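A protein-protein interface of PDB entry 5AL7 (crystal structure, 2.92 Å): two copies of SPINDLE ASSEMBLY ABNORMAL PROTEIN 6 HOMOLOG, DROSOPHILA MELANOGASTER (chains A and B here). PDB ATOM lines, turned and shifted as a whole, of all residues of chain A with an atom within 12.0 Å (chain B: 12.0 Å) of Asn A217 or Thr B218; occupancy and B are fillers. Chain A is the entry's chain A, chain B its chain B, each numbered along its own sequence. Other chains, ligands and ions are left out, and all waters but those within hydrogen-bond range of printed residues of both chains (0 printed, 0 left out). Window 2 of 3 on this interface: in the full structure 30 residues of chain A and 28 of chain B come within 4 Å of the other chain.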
ATOM      1  N   ASN A 209      -1.898 -15.947   7.782  1.00  0.00           N
ATOM      2  CA  ASN A 209      -2.303 -16.398   6.450  1.00  0.00           C
ATOM      3  C   ASN A 209      -1.251 -16.142   5.360  1.00  0.00           C
ATOM      4  O   ASN A 209      -1.361 -16.665   4.250  1.00  0.00           O
ATOM      5  CB  ASN A 209      -3.624 -15.733   6.057  1.00  0.00           C
ATOM      6  CG  ASN A 209      -4.627 -16.719   5.488  1.00  0.00           C
ATOM      7  OD1 ASN A 209      -5.206 -17.523   6.217  1.00  0.00           O
ATOM      8  ND2 ASN A 209      -4.848 -16.651   4.180  1.00  0.00           N
ATOM      9  N   LEU A 210      -0.244 -15.333   5.678  1.00  0.00           N
ATOM     10  CA  LEU A 210       0.798 -14.970   4.716  1.00  0.00           C
ATOM     11  C   LEU A 210       1.862 -16.060   4.605  1.00  0.00           C
ATOM     12  O   LEU A 210       2.515 -16.215   3.565  1.00  0.00           O
ATOM     13  CB  LEU A 210       1.450 -13.646   5.131  1.00  0.00           C
ATOM     14  CG  LEU A 210       2.550 -13.024   4.267  1.00  0.00           C
ATOM     15  CD1 LEU A 210       1.950 -12.252   3.106  1.00  0.00           C
ATOM     16  CD2 LEU A 210       3.449 -12.125   5.106  1.00  0.00           C
ATOM     17  N   ARG A 211       2.018 -16.819   5.684  1.00  0.00           N
ATOM     18  CA  ARG A 211       2.926 -17.959   5.721  1.00  0.00           C
ATOM     19  C   ARG A 211       2.431 -19.104   4.833  1.00  0.00           C
ATOM     20  O   ARG A 211       3.233 -19.853   4.275  1.00  0.00           O
ATOM     21  CB  ARG A 211       3.122 -18.420   7.167  1.00  0.00           C
ATOM     22  CG  ARG A 211       4.029 -17.480   7.950  1.00  0.00           C
ATOM     23  CD  ARG A 211       4.016 -17.748   9.443  1.00  0.00           C
ATOM     24  NE  ARG A 211       4.802 -16.747  10.161  1.00  0.00           N
ATOM     25  CZ  ARG A 211       4.493 -16.272  11.363  1.00  0.00           C
ATOM     26  NH1 ARG A 211       3.405 -16.698  11.988  1.00  0.00           N
ATOM     27  NH2 ARG A 211       5.268 -15.362  11.936  1.00  0.00           N
ATOM     28  N   GLU A 212       1.113 -19.247   4.722  1.00  0.00           N
ATOM     29  CA  GLU A 212       0.522 -20.251   3.839  1.00  0.00           C
ATOM     30  C   GLU A 212       0.678 -19.829   2.377  1.00  0.00           C
ATOM     31  O   GLU A 212       0.796 -20.672   1.486  1.00  0.00           O
ATOM     32  CB  GLU A 212      -0.954 -20.466   4.176  1.00  0.00           C
ATOM     33  CG  GLU A 212      -1.195 -21.202   5.481  1.00  0.00           C
ATOM     34  CD  GLU A 212      -2.636 -21.109   5.937  1.00  0.00           C
ATOM     35  OE1 GLU A 212      -3.497 -20.739   5.112  1.00  0.00           O
ATOM     36  OE2 GLU A 212      -2.911 -21.406   7.117  1.00  0.00           O
ATOM     37  N   ALA A 213       0.667 -18.519   2.142  1.00  0.00           N
ATOM     38  CA  ALA A 213       0.927 -17.960   0.819  1.00  0.00           C
ATOM     39  C   ALA A 213       2.385 -18.198   0.447  1.00  0.00           C
ATOM     40  O   ALA A 213       2.713 -18.442  -0.714  1.00  0.00           O
ATOM     41  CB  ALA A 213       0.599 -16.475   0.784  1.00  0.00           C
ATOM     42  N   LEU A 214       3.254 -18.112   1.450  1.00  0.00           N
ATOM     43  CA  LEU A 214       4.682 -18.357   1.276  1.00  0.00           C
ATOM     44  C   LEU A 214       4.960 -19.853   1.105  1.00  0.00           C
ATOM     45  O   LEU A 214       5.965 -20.245   0.512  1.00  0.00           O
ATOM     46  CB  LEU A 214       5.474 -17.803   2.468  1.00  0.00           C
ATOM     47  CG  LEU A 214       6.990 -17.641   2.302  1.00  0.00           C
ATOM     48  CD1 LEU A 214       7.328 -16.298   1.674  1.00  0.00           C
ATOM     49  CD2 LEU A 214       7.713 -17.808   3.632  1.00  0.00           C
ATOM     50  N   ALA A 215       4.059 -20.680   1.631  1.00  0.00           N
ATOM     51  CA  ALA A 215       4.186 -22.136   1.568  1.00  0.00           C
ATOM     52  C   ALA A 215       4.082 -22.713   0.155  1.00  0.00           C
ATOM     53  O   ALA A 215       4.745 -23.703  -0.158  1.00  0.00           O
ATOM     54  CB  ALA A 215       3.138 -22.786   2.465  1.00  0.00           C
ATOM     55  N   GLU A 216       3.256 -22.111  -0.695  1.00  0.00           N
ATOM     56  CA  GLU A 216       3.060 -22.658  -2.032  1.00  0.00           C
ATOM     57  C   GLU A 216       4.275 -22.371  -2.914  1.00  0.00           C
ATOM     58  O   GLU A 216       4.614 -23.160  -3.796  1.00  0.00           O
ATOM     59  CB  GLU A 216       1.793 -22.071  -2.662  1.00  0.00           C
ATOM     60  CG  GLU A 216       0.583 -22.046  -1.733  1.00  0.00           C
ATOM     61  CD  GLU A 216      -0.003 -23.423  -1.487  1.00  0.00           C
ATOM     62  OE1 GLU A 216      -0.326 -24.117  -2.474  1.00  0.00           O
ATOM     63  OE2 GLU A 216      -0.138 -23.813  -0.308  1.00  0.00           O
ATOM     64  N   ASN A 217       4.916 -21.232  -2.676  1.00  0.00           N
ATOM     65  CA  ASN A 217       6.150 -20.871  -3.368  1.00  0.00           C
ATOM     66  C   ASN A 217       7.394 -20.961  -2.467  1.00  0.00           C
ATOM     67  O   ASN A 217       8.221 -20.048  -2.457  1.00  0.00           O
ATOM     68  CB  ASN A 217       6.012 -19.476  -3.993  1.00  0.00           C
ATOM     69  CG  ASN A 217       5.646 -18.404  -2.982  1.00  0.00           C
ATOM     70  OD1 ASN A 217       6.008 -18.479  -1.809  1.00  0.00           O
ATOM     71  ND2 ASN A 217       4.905 -17.400  -3.439  1.00  0.00           N
ATOM     72  N   THR A 218       7.530 -22.058  -1.725  1.00  0.00           N
ATOM     73  CA  THR A 218       8.678 -22.244  -0.833  1.00  0.00           C
ATOM     74  C   THR A 218       9.708 -23.193  -1.433  1.00  0.00           C
ATOM     75  O   THR A 218      10.910 -23.032  -1.204  1.00  0.00           O
ATOM     76  CB  THR A 218       8.241 -22.785   0.553  1.00  0.00           C
ATOM     77  OG1 THR A 218       7.388 -21.831   1.195  1.00  0.00           O
ATOM     78  CG2 THR A 218       9.448 -23.044   1.451  1.00  0.00           C
ATOM     79  N   ARG A 219       9.228 -24.168  -2.206  1.00  0.00           N
ATOM     80  CA  ARG A 219      10.087 -25.165  -2.847  1.00  0.00           C
ATOM     81  C   ARG A 219      10.838 -26.084  -1.885  1.00  0.00           C
ATOM     82  O   ARG A 219      11.561 -25.649  -0.991  1.00  0.00           O
ATOM     83  CB  ARG A 219      11.090 -24.476  -3.762  1.00  0.00           C
ATOM     84  CG  ARG A 219      12.027 -25.421  -4.449  1.00  0.00           C
ATOM     85  CD  ARG A 219      13.041 -24.611  -5.175  1.00  0.00           C
ATOM     86  NE  ARG A 219      14.031 -24.022  -4.275  1.00  0.00           N
ATOM     87  CZ  ARG A 219      15.145 -24.626  -3.874  1.00  0.00           C
ATOM     88  NH1 ARG A 219      15.434 -25.847  -4.302  1.00  0.00           N
ATOM     89  NH2 ARG A 219      15.980 -24.001  -3.054  1.00  0.00           N
ATOM     90  OXT ARG A 219      10.740 -27.306  -1.995  1.00  0.00           O
ATOM     91  N   ASN B 209       9.593  -8.362   7.115  1.00  0.00           N
ATOM     92  CA  ASN B 209      10.578  -9.143   6.376  1.00  0.00           C
ATOM     93  C   ASN B 209       9.910 -10.282   5.612  1.00  0.00           C
ATOM     94  O   ASN B 209      10.471 -10.824   4.649  1.00  0.00           O
ATOM     95  CB  ASN B 209      11.641  -9.690   7.331  1.00  0.00           C
ATOM     96  CG  ASN B 209      12.363  -8.592   8.090  1.00  0.00           C
ATOM     97  OD1 ASN B 209      11.774  -7.911   8.927  1.00  0.00           O
ATOM     98  ND2 ASN B 209      13.649  -8.422   7.804  1.00  0.00           N
ATOM     99  N   LEU B 210       8.692 -10.622   6.022  1.00  0.00           N
ATOM    100  CA  LEU B 210       7.944 -11.674   5.350  1.00  0.00           C
ATOM    101  C   LEU B 210       7.184 -11.089   4.154  1.00  0.00           C
ATOM    102  O   LEU B 210       6.890 -11.806   3.190  1.00  0.00           O
ATOM    103  CB  LEU B 210       7.007 -12.396   6.322  1.00  0.00           C
ATOM    104  CG  LEU B 210       7.713 -13.431   7.210  1.00  0.00           C
ATOM    105  CD1 LEU B 210       6.712 -14.372   7.866  1.00  0.00           C
ATOM    106  CD2 LEU B 210       8.762 -14.219   6.431  1.00  0.00           C
ATOM    107  N   ARG B 211       6.871  -9.792   4.207  1.00  0.00           N
ATOM    108  CA  ARG B 211       6.285  -9.139   3.037  1.00  0.00           C
ATOM    109  C   ARG B 211       7.328  -9.071   1.930  1.00  0.00           C
ATOM    110  O   ARG B 211       7.004  -9.188   0.748  1.00  0.00           O
ATOM    111  CB  ARG B 211       5.808  -7.717   3.340  1.00  0.00           C
ATOM    112  CG  ARG B 211       4.524  -7.575   4.124  1.00  0.00           C
ATOM    113  CD  ARG B 211       4.359  -6.111   4.495  1.00  0.00           C
ATOM    114  NE  ARG B 211       3.209  -5.849   5.350  1.00  0.00           N
ATOM    115  CZ  ARG B 211       3.187  -4.914   6.293  1.00  0.00           C
ATOM    116  NH1 ARG B 211       4.257  -4.160   6.508  1.00  0.00           N
ATOM    117  NH2 ARG B 211       2.100  -4.739   7.030  1.00  0.00           N
ATOM    118  N   GLU B 212       8.580  -8.861   2.333  1.00  0.00           N
ATOM    119  CA  GLU B 212       9.714  -8.823   1.412  1.00  0.00           C
ATOM    120  C   GLU B 212      10.098 -10.220   0.927  1.00  0.00           C
ATOM    121  O   GLU B 212      10.584 -10.379  -0.193  1.00  0.00           O
ATOM    122  CB  GLU B 212      10.920  -8.140   2.071  1.00  0.00           C
ATOM    123  CG  GLU B 212      10.766  -6.629   2.241  1.00  0.00           C
ATOM    124  CD  GLU B 212      11.812  -6.026   3.166  1.00  0.00           C
ATOM    125  OE1 GLU B 212      12.829  -6.696   3.442  1.00  0.00           O
ATOM    126  OE2 GLU B 212      11.616  -4.876   3.614  1.00  0.00           O
ATOM    127  N   ALA B 213       9.897 -11.228   1.774  1.00  0.00           N
ATOM    128  CA  ALA B 213      10.123 -12.605   1.345  1.00  0.00           C
ATOM    129  C   ALA B 213       9.074 -13.010   0.306  1.00  0.00           C
ATOM    130  O   ALA B 213       9.389 -13.679  -0.691  1.00  0.00           O
ATOM    131  CB  ALA B 213      10.094 -13.551   2.538  1.00  0.00           C
ATOM    132  N   LEU B 214       7.835 -12.565   0.520  1.00  0.00           N
ATOM    133  CA  LEU B 214       6.757 -12.869  -0.417  1.00  0.00           C
ATOM    134  C   LEU B 214       6.902 -12.039  -1.688  1.00  0.00           C
ATOM    135  O   LEU B 214       6.454 -12.447  -2.758  1.00  0.00           O
ATOM    136  CB  LEU B 214       5.387 -12.622   0.217  1.00  0.00           C
ATOM    137  CG  LEU B 214       4.213 -13.249  -0.542  1.00  0.00           C
ATOM    138  CD1 LEU B 214       3.994 -14.692  -0.111  1.00  0.00           C
ATOM    139  CD2 LEU B 214       2.945 -12.432  -0.367  1.00  0.00           C
ATOM    140  N   ALA B 215       7.496 -10.856  -1.567  1.00  0.00           N
ATOM    141  CA  ALA B 215       7.764 -10.030  -2.738  1.00  0.00           C
ATOM    142  C   ALA B 215       8.886 -10.653  -3.571  1.00  0.00           C
ATOM    143  O   ALA B 215       8.858 -10.620  -4.800  1.00  0.00           O
ATOM    144  CB  ALA B 215       8.124  -8.611  -2.324  1.00  0.00           C
ATOM    145  N   GLU B 216       9.871 -11.221  -2.877  1.00  0.00           N
ATOM    146  CA  GLU B 216      11.050 -11.812  -3.512  1.00  0.00           C
ATOM    147  C   GLU B 216      10.810 -13.195  -4.119  1.00  0.00           C
ATOM    148  O   GLU B 216      11.514 -13.583  -5.050  1.00  0.00           O
ATOM    149  CB  GLU B 216      12.220 -11.886  -2.523  1.00  0.00           C
ATOM    150  CG  GLU B 216      13.567 -12.145  -3.199  1.00  0.00           C
ATOM    151  CD  GLU B 216      14.734 -12.168  -2.231  1.00  0.00           C
ATOM    152  OE1 GLU B 216      14.586 -11.653  -1.102  1.00  0.00           O
ATOM    153  OE2 GLU B 216      15.803 -12.702  -2.601  1.00  0.00           O
ATOM    154  N   ASN B 217       9.822 -13.940  -3.629  1.00  0.00           N
ATOM    155  CA  ASN B 217       9.618 -15.278  -4.186  1.00  0.00           C
ATOM    156  C   ASN B 217       8.865 -15.240  -5.514  1.00  0.00           C
ATOM    157  O   ASN B 217       9.112 -16.060  -6.398  1.00  0.00           O
ATOM    158  CB  ASN B 217       8.874 -16.181  -3.189  1.00  0.00           C
ATOM    159  CG  ASN B 217       7.499 -15.644  -2.805  1.00  0.00           C
ATOM    160  OD1 ASN B 217       6.827 -14.980  -3.593  1.00  0.00           O
ATOM    161  ND2 ASN B 217       7.072 -15.943  -1.584  1.00  0.00           N
ATOM    162  N   THR B 218       7.942 -14.293  -5.649  1.00  0.00           N
ATOM    163  CA  THR B 218       7.210 -14.116  -6.898  1.00  0.00           C
ATOM    164  C   THR B 218       7.685 -12.882  -7.673  1.00  0.00           C
ATOM    165  O   THR B 218       6.899 -12.262  -8.391  1.00  0.00           O
ATOM    166  CB  THR B 218       5.689 -14.002  -6.654  1.00  0.00           C
ATOM    167  OG1 THR B 218       5.440 -13.087  -5.578  1.00  0.00           O
ATOM    168  CG2 THR B 218       5.099 -15.361  -6.303  1.00  0.00           C
ATOM    169  N   ARG B 219       8.961 -12.523  -7.534  1.00  0.00           N
ATOM    170  CA  ARG B 219       9.479 -11.325  -8.199  1.00  0.00           C
ATOM    171  C   ARG B 219       9.618 -11.573  -9.703  1.00  0.00           C
ATOM    172  O   ARG B 219      10.277 -12.520 -10.137  1.00  0.00           O
ATOM    173  CB  ARG B 219      10.831 -10.893  -7.605  1.00  0.00           C
ATOM    174  CG  ARG B 219      11.353  -9.560  -8.163  1.00  0.00           C
ATOM    175  CD  ARG B 219      12.766  -9.214  -7.694  1.00  0.00           C
ATOM    176  NE  ARG B 219      13.794  -9.934  -8.442  1.00  0.00           N
ATOM    177  CZ  ARG B 219      14.312  -9.506  -9.591  1.00  0.00           C
ATOM    178  NH1 ARG B 219      13.903  -8.360 -10.115  1.00  0.00           N
ATOM    179  NH2 ARG B 219      15.241 -10.218 -10.213  1.00  0.00           N
ATOM    180  OXT ARG B 219       9.070 -10.834 -10.523  1.00  0.00           O
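The side-chain amide oxygen (OD1) of Asn A217 is in hydrogen-bond range of the side-chain amide nitrogen (ND2) of Asn B217 (2.8 Å).
The side-chain amide oxygen (OD1) of Asn B217 lies close to the backbone carbonyl oxygen (O) of Leu B214.
O of Ala B213 sits at hydrogen-bond distance from ND2 of Asn B217 (3.4 Å).
OD1 of Asn A217 lies close to O of Ala A213, at 3.5 Å.
The side-chain hydroxyl (OG1) of Thr B218 lies within hydrogen-bond range of the backbone carbonyl oxygen (O) of Leu B214, 3.1 Å away.
The side-chain amide oxygen (OD1) of Asn B217 sits at hydrogen-bond distance from the side-chain hydroxyl (OG1) of Thr B218.
The backbone carbonyl oxygen of Leu A214 sits close to the side-chain amide oxygen of Asn A217 (2.9 Å).
Leu B210 touches Leu A210.
CD1 of Leu A210 touches CD2 of Leu B214, 3.6 Å away.
Arg A211 touches Leu B210.
Ala A213 touches Leu B214.
CD1 of Leu A214 touches C of Ala B213 (3.97 Å).
Leu A214 touches Leu B214 (N to CD1, 3.8 Å).
Leu A214 touches Asn B217 (CD1 to ND2, 3.3 Å).
CG2 of Thr B218 touches ND2 of Asn A217, at 3.5 Å.
Of chain B, only Asn B217 and Thr B218 come within 4 Å of Asn A217.
Thr B218 touches just one residue of chain A: Asn A217 (3.5 Å).
Of chain B, only Leu B214 comes within 4 Å of Ala A213.
Leu A214 touches just these residues of chain B: Ala B213 (3.97 Å), Leu B214 (3.8 Å) and Asn B217 (3.3 Å).
Ala A215 touches none of the printed residues of chain B.
No residue of chain B comes within 4 Å of Glu A216.
No residue of chain B comes within 4 Å of Thr A218.
Leu B214 touches just these residues of chain A: Leu A210 (3.6 Å), Ala A213 (3.9 Å) and Leu A214 (3.8 Å).
Asn B217 touches just these residues of chain A: Leu A214 and Asn A217.
Printed residues of chain A within 4 Å of Ala B213: Leu A214.
Of the printed residues of chain A, Leu B210 touches Leu A210 (3.8 Å) and Arg A211 (3.8 Å).
Of the printed residues of chain B, Leu A210 touches Leu B210 (3.8 Å) and Leu B214 (3.6 Å).
Of the printed residues of chain B, Arg A211 touches Leu B210.
The nearest residue of chain B that does not touch Asn A217 is Leu B214 (4.4 Å).
Printed residues of chain B that touch a printed residue of chain A: Leu B210, Ala B213, Leu B214, Asn B217 and Thr B218.
Among the printed residues, 9 pairs touch across the chains.
Leu A210 touches Leu B214, but with the chains exchanged Leu A214 does not touch Leu B210 (4.7 Å).
Arg A211 touches Leu B210, but with the chains exchanged Leu A210 does not touch Arg B211 (4.2 Å).
Leu A214 touches Asn B217, but with the chains exchanged Asn A217 does not touch Leu B214 (4.4 Å).
Asn A217 touches its own counterpart, Asn B217.
Positions printed for both chains: 209, 210, 211, 212, 213, 214, 215, 216, 217, 218 and 219.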
